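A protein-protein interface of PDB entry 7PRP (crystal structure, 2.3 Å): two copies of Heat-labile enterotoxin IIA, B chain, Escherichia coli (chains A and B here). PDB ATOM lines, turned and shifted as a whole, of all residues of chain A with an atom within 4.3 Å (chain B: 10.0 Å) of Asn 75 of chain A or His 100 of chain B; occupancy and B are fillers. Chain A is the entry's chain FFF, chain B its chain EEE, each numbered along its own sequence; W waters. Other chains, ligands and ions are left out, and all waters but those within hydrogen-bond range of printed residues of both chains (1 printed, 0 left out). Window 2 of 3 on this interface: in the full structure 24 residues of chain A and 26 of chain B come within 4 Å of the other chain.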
ATOM      1  N   GLN A  22     -14.540  16.343  23.008  1.00  0.00           N
ATOM      2  CA  GLN A  22     -13.657  17.078  22.065  1.00  0.00           C
ATOM      3  C   GLN A  22     -14.240  18.479  21.780  1.00  0.00           C
ATOM      4  O   GLN A  22     -15.304  18.616  21.179  1.00  0.00           O
ATOM      5  CB  GLN A  22     -13.395  16.345  20.749  1.00  0.00           C
ATOM      6  CG  GLN A  22     -12.228  16.988  19.974  1.00  0.00           C
ATOM      7  CD  GLN A  22     -11.014  17.188  20.874  1.00  0.00           C
ATOM      8  OE1 GLN A  22     -10.342  16.220  21.281  1.00  0.00           O
ATOM      9  NE2 GLN A  22     -10.715  18.446  21.208  1.00  0.00           N
ATOM     10  N   VAL A  24     -14.206  21.871  19.686  1.00  0.00           N
ATOM     11  CA  VAL A  24     -13.850  22.279  18.296  1.00  0.00           C
ATOM     12  C   VAL A  24     -13.998  23.793  18.109  1.00  0.00           C
ATOM     13  O   VAL A  24     -13.518  24.297  17.072  1.00  0.00           O
ATOM     14  CB  VAL A  24     -14.713  21.493  17.306  1.00  0.00           C
ATOM     15  CG1 VAL A  24     -14.403  20.003  17.391  1.00  0.00           C
ATOM     16  CG2 VAL A  24     -16.202  21.741  17.495  1.00  0.00           C
ATOM     17  N   ALA A  70      -6.207  25.331  24.701  1.00  0.00           N
ATOM     18  CA  ALA A  70      -5.244  24.271  24.337  1.00  0.00           C
ATOM     19  C   ALA A  70      -5.992  23.054  23.780  1.00  0.00           C
ATOM     20  O   ALA A  70      -5.479  22.406  22.875  1.00  0.00           O
ATOM     21  CB  ALA A  70      -4.425  23.874  25.542  1.00  0.00           C
ATOM     22  N   ALA A  71      -7.120  22.704  24.370  1.00  0.00           N
ATOM     23  CA  ALA A  71      -7.928  21.574  23.891  1.00  0.00           C
ATOM     24  C   ALA A  71      -8.370  21.821  22.448  1.00  0.00           C
ATOM     25  O   ALA A  71      -8.316  20.903  21.683  1.00  0.00           O
ATOM     26  CB  ALA A  71      -9.102  21.353  24.794  1.00  0.00           C
ATOM     27  N   VAL A  72      -8.844  23.014  22.116  1.00  0.00           N
ATOM     28  CA  VAL A  72      -9.328  23.314  20.742  1.00  0.00           C
ATOM     29  C   VAL A  72      -8.139  23.342  19.795  1.00  0.00           C
ATOM     30  O   VAL A  72      -8.185  22.691  18.777  1.00  0.00           O
ATOM     31  CB  VAL A  72     -10.140  24.617  20.689  1.00  0.00           C
ATOM     32  CG1 VAL A  72     -10.525  24.966  19.254  1.00  0.00           C
ATOM     33  CG2 VAL A  72     -11.399  24.521  21.576  1.00  0.00           C
ATOM     34  N   LEU A  73      -7.080  24.036  20.157  1.00  0.00           N
ATOM     35  CA  LEU A  73      -5.922  24.249  19.257  1.00  0.00           C
ATOM     36  C   LEU A  73      -5.163  22.945  19.035  1.00  0.00           C
ATOM     37  O   LEU A  73      -4.722  22.733  17.921  1.00  0.00           O
ATOM     38  CB  LEU A  73      -5.035  25.327  19.898  1.00  0.00           C
ATOM     39  CG  LEU A  73      -4.037  25.988  18.965  1.00  0.00           C
ATOM     40  CD1 LEU A  73      -4.723  26.548  17.720  1.00  0.00           C
ATOM     41  CD2 LEU A  73      -3.249  27.060  19.730  1.00  0.00           C
ATOM     42  N   SER A  74      -5.019  22.108  20.052  1.00  0.00           N
ATOM     43  CA  SER A  74      -4.254  20.838  19.958  1.00  0.00           C
ATOM     44  C   SER A  74      -5.185  19.647  19.700  1.00  0.00           C
ATOM     45  O   SER A  74      -4.670  18.563  19.562  1.00  0.00           O
ATOM     46  CB  SER A  74      -3.414  20.614  21.186  1.00  0.00           C
ATOM     47  OG  SER A  74      -2.550  21.715  21.409  1.00  0.00           O
ATOM     48  N   ASN A  75      -6.494  19.847  19.601  1.00  0.00           N
ATOM     49  CA  ASN A  75      -7.472  18.740  19.394  1.00  0.00           C
ATOM     50  C   ASN A  75      -7.248  17.677  20.484  1.00  0.00           C
ATOM     51  O   ASN A  75      -7.059  16.492  20.159  1.00  0.00           O
ATOM     52  CB  ASN A  75      -7.370  18.169  17.983  1.00  0.00           C
ATOM     53  CG  ASN A  75      -8.512  17.254  17.618  1.00  0.00           C
ATOM     54  OD1 ASN A  75      -9.677  17.664  17.652  1.00  0.00           O
ATOM     55  ND2 ASN A  75      -8.164  16.036  17.231  1.00  0.00           N
ATOM     56  N   VAL A  76      -7.308  18.096  21.745  1.00  0.00           N
ATOM     57  CA  VAL A  76      -7.088  17.238  22.942  1.00  0.00           C
ATOM     58  C   VAL A  76      -8.390  17.234  23.733  1.00  0.00           C
ATOM     59  O   VAL A  76      -9.029  18.301  23.834  1.00  0.00           O
ATOM     60  CB  VAL A  76      -5.890  17.779  23.753  1.00  0.00           C
ATOM     61  CG1 VAL A  76      -5.865  17.279  25.184  1.00  0.00           C
ATOM     62  CG2 VAL A  76      -4.590  17.429  23.059  1.00  0.00           C
ATOM     63  N   GLY B   1     -15.499  24.731  11.807  1.00  0.00           N
ATOM     64  CA  GLY B   1     -16.814  25.260  11.388  1.00  0.00           C
ATOM     65  C   GLY B   1     -17.289  26.343  12.333  1.00  0.00           C
ATOM     66  O   GLY B   1     -16.496  26.826  13.166  1.00  0.00           O
ATOM     67  N   VAL B   2     -18.556  26.705  12.247  1.00  0.00           N
ATOM     68  CA  VAL B   2     -19.147  27.769  13.101  1.00  0.00           C
ATOM     69  C   VAL B   2     -20.101  27.113  14.079  1.00  0.00           C
ATOM     70  O   VAL B   2     -20.910  26.334  13.577  1.00  0.00           O
ATOM     71  CB  VAL B   2     -19.978  28.717  12.243  1.00  0.00           C
ATOM     72  CG1 VAL B   2     -20.309  29.985  13.001  1.00  0.00           C
ATOM     73  CG2 VAL B   2     -19.363  28.935  10.884  1.00  0.00           C
ATOM     74  N   SER B  20     -15.256  31.306   8.471  1.00  0.00           N
ATOM     75  CA  SER B  20     -14.124  30.622   7.842  1.00  0.00           C
ATOM     76  C   SER B  20     -13.157  31.669   7.247  1.00  0.00           C
ATOM     77  O   SER B  20     -12.860  31.623   6.010  1.00  0.00           O
ATOM     78  CB  SER B  20     -14.662  29.673   6.795  1.00  0.00           C
ATOM     79  OG  SER B  20     -13.694  28.674   6.522  1.00  0.00           O
ATOM     80  N   VAL B  76      -4.917  28.650  11.366  1.00  0.00           N
ATOM     81  CA  VAL B  76      -6.220  28.061  11.789  1.00  0.00           C
ATOM     82  C   VAL B  76      -7.302  29.102  11.509  1.00  0.00           C
ATOM     83  O   VAL B  76      -7.061  30.281  11.777  1.00  0.00           O
ATOM     84  CB  VAL B  76      -6.174  27.642  13.279  1.00  0.00           C
ATOM     85  CG1 VAL B  76      -7.535  27.362  13.838  1.00  0.00           C
ATOM     86  CG2 VAL B  76      -5.317  26.412  13.462  1.00  0.00           C
ATOM     87  N   ARG B  77      -8.463  28.664  11.033  1.00  0.00           N
ATOM     88  CA  ARG B  77      -9.598  29.538  10.679  1.00  0.00           C
ATOM     89  C   ARG B  77     -10.245  30.127  11.943  1.00  0.00           C
ATOM     90  O   ARG B  77     -10.152  29.512  13.031  1.00  0.00           O
ATOM     91  CB  ARG B  77     -10.540  28.765   9.747  1.00  0.00           C
ATOM     92  CG  ARG B  77     -10.186  28.891   8.264  1.00  0.00           C
ATOM     93  CD  ARG B  77     -10.081  27.656   7.376  1.00  0.00           C
ATOM     94  NE  ARG B  77     -10.852  27.804   6.141  1.00  0.00           N
ATOM     95  CZ  ARG B  77     -10.508  28.523   5.055  1.00  0.00           C
ATOM     96  NH1 ARG B  77     -11.367  28.609   4.046  1.00  0.00           N
ATOM     97  NH2 ARG B  77      -9.331  29.133   4.955  1.00  0.00           N
ATOM     98  N   LEU B  96     -12.389  30.602  17.487  1.00  0.00           N
ATOM     99  CA  LEU B  96     -11.353  29.725  16.906  1.00  0.00           C
ATOM    100  C   LEU B  96     -12.077  28.538  16.296  1.00  0.00           C
ATOM    101  O   LEU B  96     -12.896  27.923  17.036  1.00  0.00           O
ATOM    102  CB  LEU B  96     -10.390  29.312  18.013  1.00  0.00           C
ATOM    103  CG  LEU B  96      -9.128  28.628  17.529  1.00  0.00           C
ATOM    104  CD1 LEU B  96      -8.293  29.587  16.734  1.00  0.00           C
ATOM    105  CD2 LEU B  96      -8.352  28.011  18.665  1.00  0.00           C
ATOM    106  N   ALA B  97     -11.800  28.232  15.022  1.00  0.00           N
ATOM    107  CA  ALA B  97     -12.590  27.319  14.180  1.00  0.00           C
ATOM    108  C   ALA B  97     -11.657  26.422  13.364  1.00  0.00           C
ATOM    109  O   ALA B  97     -11.617  26.526  12.148  1.00  0.00           O
ATOM    110  CB  ALA B  97     -13.496  28.146  13.310  1.00  0.00           C
ATOM    111  N   PRO B  98     -10.862  25.545  14.018  1.00  0.00           N
ATOM    112  CA  PRO B  98     -10.035  24.572  13.330  1.00  0.00           C
ATOM    113  C   PRO B  98     -10.905  23.715  12.401  1.00  0.00           C
ATOM    114  O   PRO B  98     -11.972  23.306  12.836  1.00  0.00           O
ATOM    115  CB  PRO B  98      -9.416  23.727  14.462  1.00  0.00           C
ATOM    116  CG  PRO B  98     -10.292  23.975  15.658  1.00  0.00           C
ATOM    117  CD  PRO B  98     -10.757  25.403  15.481  1.00  0.00           C
ATOM    118  N   HIS B  99     -10.467  23.505  11.155  1.00  0.00           N
ATOM    119  CA  HIS B  99     -11.243  22.740  10.153  1.00  0.00           C
ATOM    120  C   HIS B  99     -11.109  21.257  10.502  1.00  0.00           C
ATOM    121  O   HIS B  99      -9.998  20.756  10.520  1.00  0.00           O
ATOM    122  CB  HIS B  99     -10.806  23.072   8.720  1.00  0.00           C
ATOM    123  CG  HIS B  99     -11.582  22.304   7.700  1.00  0.00           C
ATOM    124  ND1 HIS B  99     -12.792  22.755   7.169  1.00  0.00           N
ATOM    125  CD2 HIS B  99     -11.344  21.103   7.127  1.00  0.00           C
ATOM    126  CE1 HIS B  99     -13.241  21.869   6.307  1.00  0.00           C
ATOM    127  NE2 HIS B  99     -12.378  20.853   6.265  1.00  0.00           N
ATOM    128  N   HIS B 100     -12.204  20.593  10.805  1.00  0.00           N
ATOM    129  CA  HIS B 100     -12.194  19.133  11.061  1.00  0.00           C
ATOM    130  C   HIS B 100     -12.914  18.432   9.909  1.00  0.00           C
ATOM    131  O   HIS B 100     -13.917  18.977   9.408  1.00  0.00           O
ATOM    132  CB  HIS B 100     -12.741  18.823  12.454  1.00  0.00           C
ATOM    133  CG  HIS B 100     -11.741  19.069  13.535  1.00  0.00           C
ATOM    134  ND1 HIS B 100     -11.652  20.272  14.206  1.00  0.00           N
ATOM    135  CD2 HIS B 100     -10.863  18.237  14.151  1.00  0.00           C
ATOM    136  CE1 HIS B 100     -10.727  20.190  15.135  1.00  0.00           C
ATOM    137  NE2 HIS B 100     -10.240  18.944  15.133  1.00  0.00           N
ATOM    138  N   HIS B 101     -12.338  17.313   9.452  1.00  0.00           N
ATOM    139  CA  HIS B 101     -12.904  16.418   8.407  1.00  0.00           C
ATOM    140  C   HIS B 101     -13.986  15.565   9.066  1.00  0.00           C
ATOM    141  O   HIS B 101     -13.760  15.066  10.205  1.00  0.00           O
ATOM    142  CB  HIS B 101     -11.781  15.602   7.714  1.00  0.00           C
ATOM    143  CG  HIS B 101     -10.868  16.440   6.868  1.00  0.00           C
ATOM    144  ND1 HIS B 101      -9.649  16.894   7.340  1.00  0.00           N
ATOM    145  CD2 HIS B 101     -11.008  16.967   5.625  1.00  0.00           C
ATOM    146  CE1 HIS B 101      -9.075  17.655   6.422  1.00  0.00           C
ATOM    147  NE2 HIS B 101      -9.887  17.715   5.364  1.00  0.00           N
ATOM    148  N   HIS B 102     -15.148  15.452   8.421  1.00  0.00           N
ATOM    149  CA  HIS B 102     -16.205  14.475   8.803  1.00  0.00           C
ATOM    150  C   HIS B 102     -16.456  13.570   7.590  1.00  0.00           C
ATOM    151  O   HIS B 102     -17.140  14.012   6.630  1.00  0.00           O
ATOM    152  CB  HIS B 102     -17.476  15.165   9.329  1.00  0.00           C
ATOM    153  CG  HIS B 102     -17.211  16.306  10.260  1.00  0.00           C
ATOM    154  ND1 HIS B 102     -16.740  16.130  11.554  1.00  0.00           N
ATOM    155  CD2 HIS B 102     -17.340  17.641  10.072  1.00  0.00           C
ATOM    156  CE1 HIS B 102     -16.588  17.314  12.119  1.00  0.00           C
ATOM    157  NE2 HIS B 102     -16.976  18.261  11.239  1.00  0.00           N
ATOM    158  N   HIS B 103     -15.904  12.349   7.618  1.00  0.00           N
ATOM    159  CA  HIS B 103     -15.998  11.380   6.509  1.00  0.00           C
ATOM    160  C   HIS B 103     -17.092  10.368   6.849  1.00  0.00           C
ATOM    161  O   HIS B 103     -16.733   9.236   7.275  1.00  0.00           O
ATOM    162  CB  HIS B 103     -14.640  10.706   6.274  1.00  0.00           C
ATOM    163  CG  HIS B 103     -13.545  11.648   5.926  1.00  0.00           C
ATOM    164  ND1 HIS B 103     -13.676  12.620   4.932  1.00  0.00           N
ATOM    165  CD2 HIS B 103     -12.293  11.742   6.416  1.00  0.00           C
ATOM    166  CE1 HIS B 103     -12.531  13.287   4.825  1.00  0.00           C
ATOM    167  NE2 HIS B 103     -11.655  12.747   5.724  1.00  0.00           N
ATOM    168  N   HIS B 104     -18.353  10.749   6.577  1.00  0.00           N
ATOM    169  CA  HIS B 104     -19.588   9.920   6.719  1.00  0.00           C
ATOM    170  C   HIS B 104     -20.693  10.446   5.796  1.00  0.00           C
ATOM    171  O   HIS B 104     -20.655  11.640   5.468  1.00  0.00           O
ATOM    172  CB  HIS B 104     -20.037   9.876   8.184  1.00  0.00           C
ATOM    173  CG  HIS B 104     -20.483  11.190   8.742  1.00  0.00           C
ATOM    174  ND1 HIS B 104     -21.771  11.405   9.216  1.00  0.00           N
ATOM    175  CD2 HIS B 104     -19.812  12.347   8.935  1.00  0.00           C
ATOM    176  CE1 HIS B 104     -21.870  12.643   9.656  1.00  0.00           C
ATOM    177  NE2 HIS B 104     -20.684  13.248   9.485  1.00  0.00           N
ATOM    178  OXT HIS B 104     -21.624   9.713   5.381  1.00  0.00           O
HETATM  179  O   HOH W   1     -13.979  24.185  14.314  1.00  0.00           O
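A ring nitrogen (NE2) of His 100 of chain B is in hydrogen-bond range of the side-chain amide oxygen (OD1) of Asn 75 of chain A.
The backbone carbonyl oxygen of Pro 98 of chain B is in hydrogen-bond range of a ring nitrogen (ND1) of His 100 of chain B. O of Asn 75 of chain A lies close to OE1 of Gln 22 of chain A (3.5 Å).
Val 24 of chain A touches Leu 96 of chain B. Pro 98 of chain B touches Val 24 of chain A. Val 72 of chain A touches Leu 96 of chain B. Val 72 of chain A touches Pro 98 of chain B.
Of the printed residues of chain B, Asn 75 of chain A touches His 100 (2.9 Å). No residue of chain B comes within 4 Å of Ser 74 of chain A. Val 76 of chain A touches none of the printed residues of chain B. Of the printed residues of chain B, Val 72 of chain A touches Leu 96 (3.8 Å) and Pro 98 (3.7 Å). Printed residues of chain A within 4 Å of Pro 98 of chain B: Val 24 (3.4 Å) and Val 72 (3.7 Å). Of the printed residues of chain B, Val 24 of chain A touches Leu 96 and Pro 98. Printed residues of chain A within 4 Å of Leu 96 of chain B: Val 24 (3.7 Å) and Val 72 (3.8 Å). Gly 1 of chain B touches none of the printed residues of chain A. The nearest printed residue of chain B that does not touch Val 72 of chain A is His 100 of chain B (5.1 Å).
Of the 14 printed residues of chain B, 3 touch a printed residue of chain A. Printed residues of chain B that touch a printed residue of chain A: Leu 96, Pro 98 and His 100. Hydrophobic or aromatic side chains of chain B that line the printed part of chain A: Leu 96, Pro 98 and His 100. Of the 9 printed residues of chain A, 3 touch a printed residue of chain B. Printed residues of chain A that touch a printed residue of chain B: Val 24, Val 72 and Asn 75. Among the printed residues, 5 pairs touch across the chains.
Position printed for both chains: 76. Of the 5 pairs that touch across the chains among the printed residues, none has its exchanged pair printed and touching as well.
Water W1 lies within hydrogen-bond range of O of Pro 98 of chain B, O of Val 24 of chain A and N of Gly 1 of chain B.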
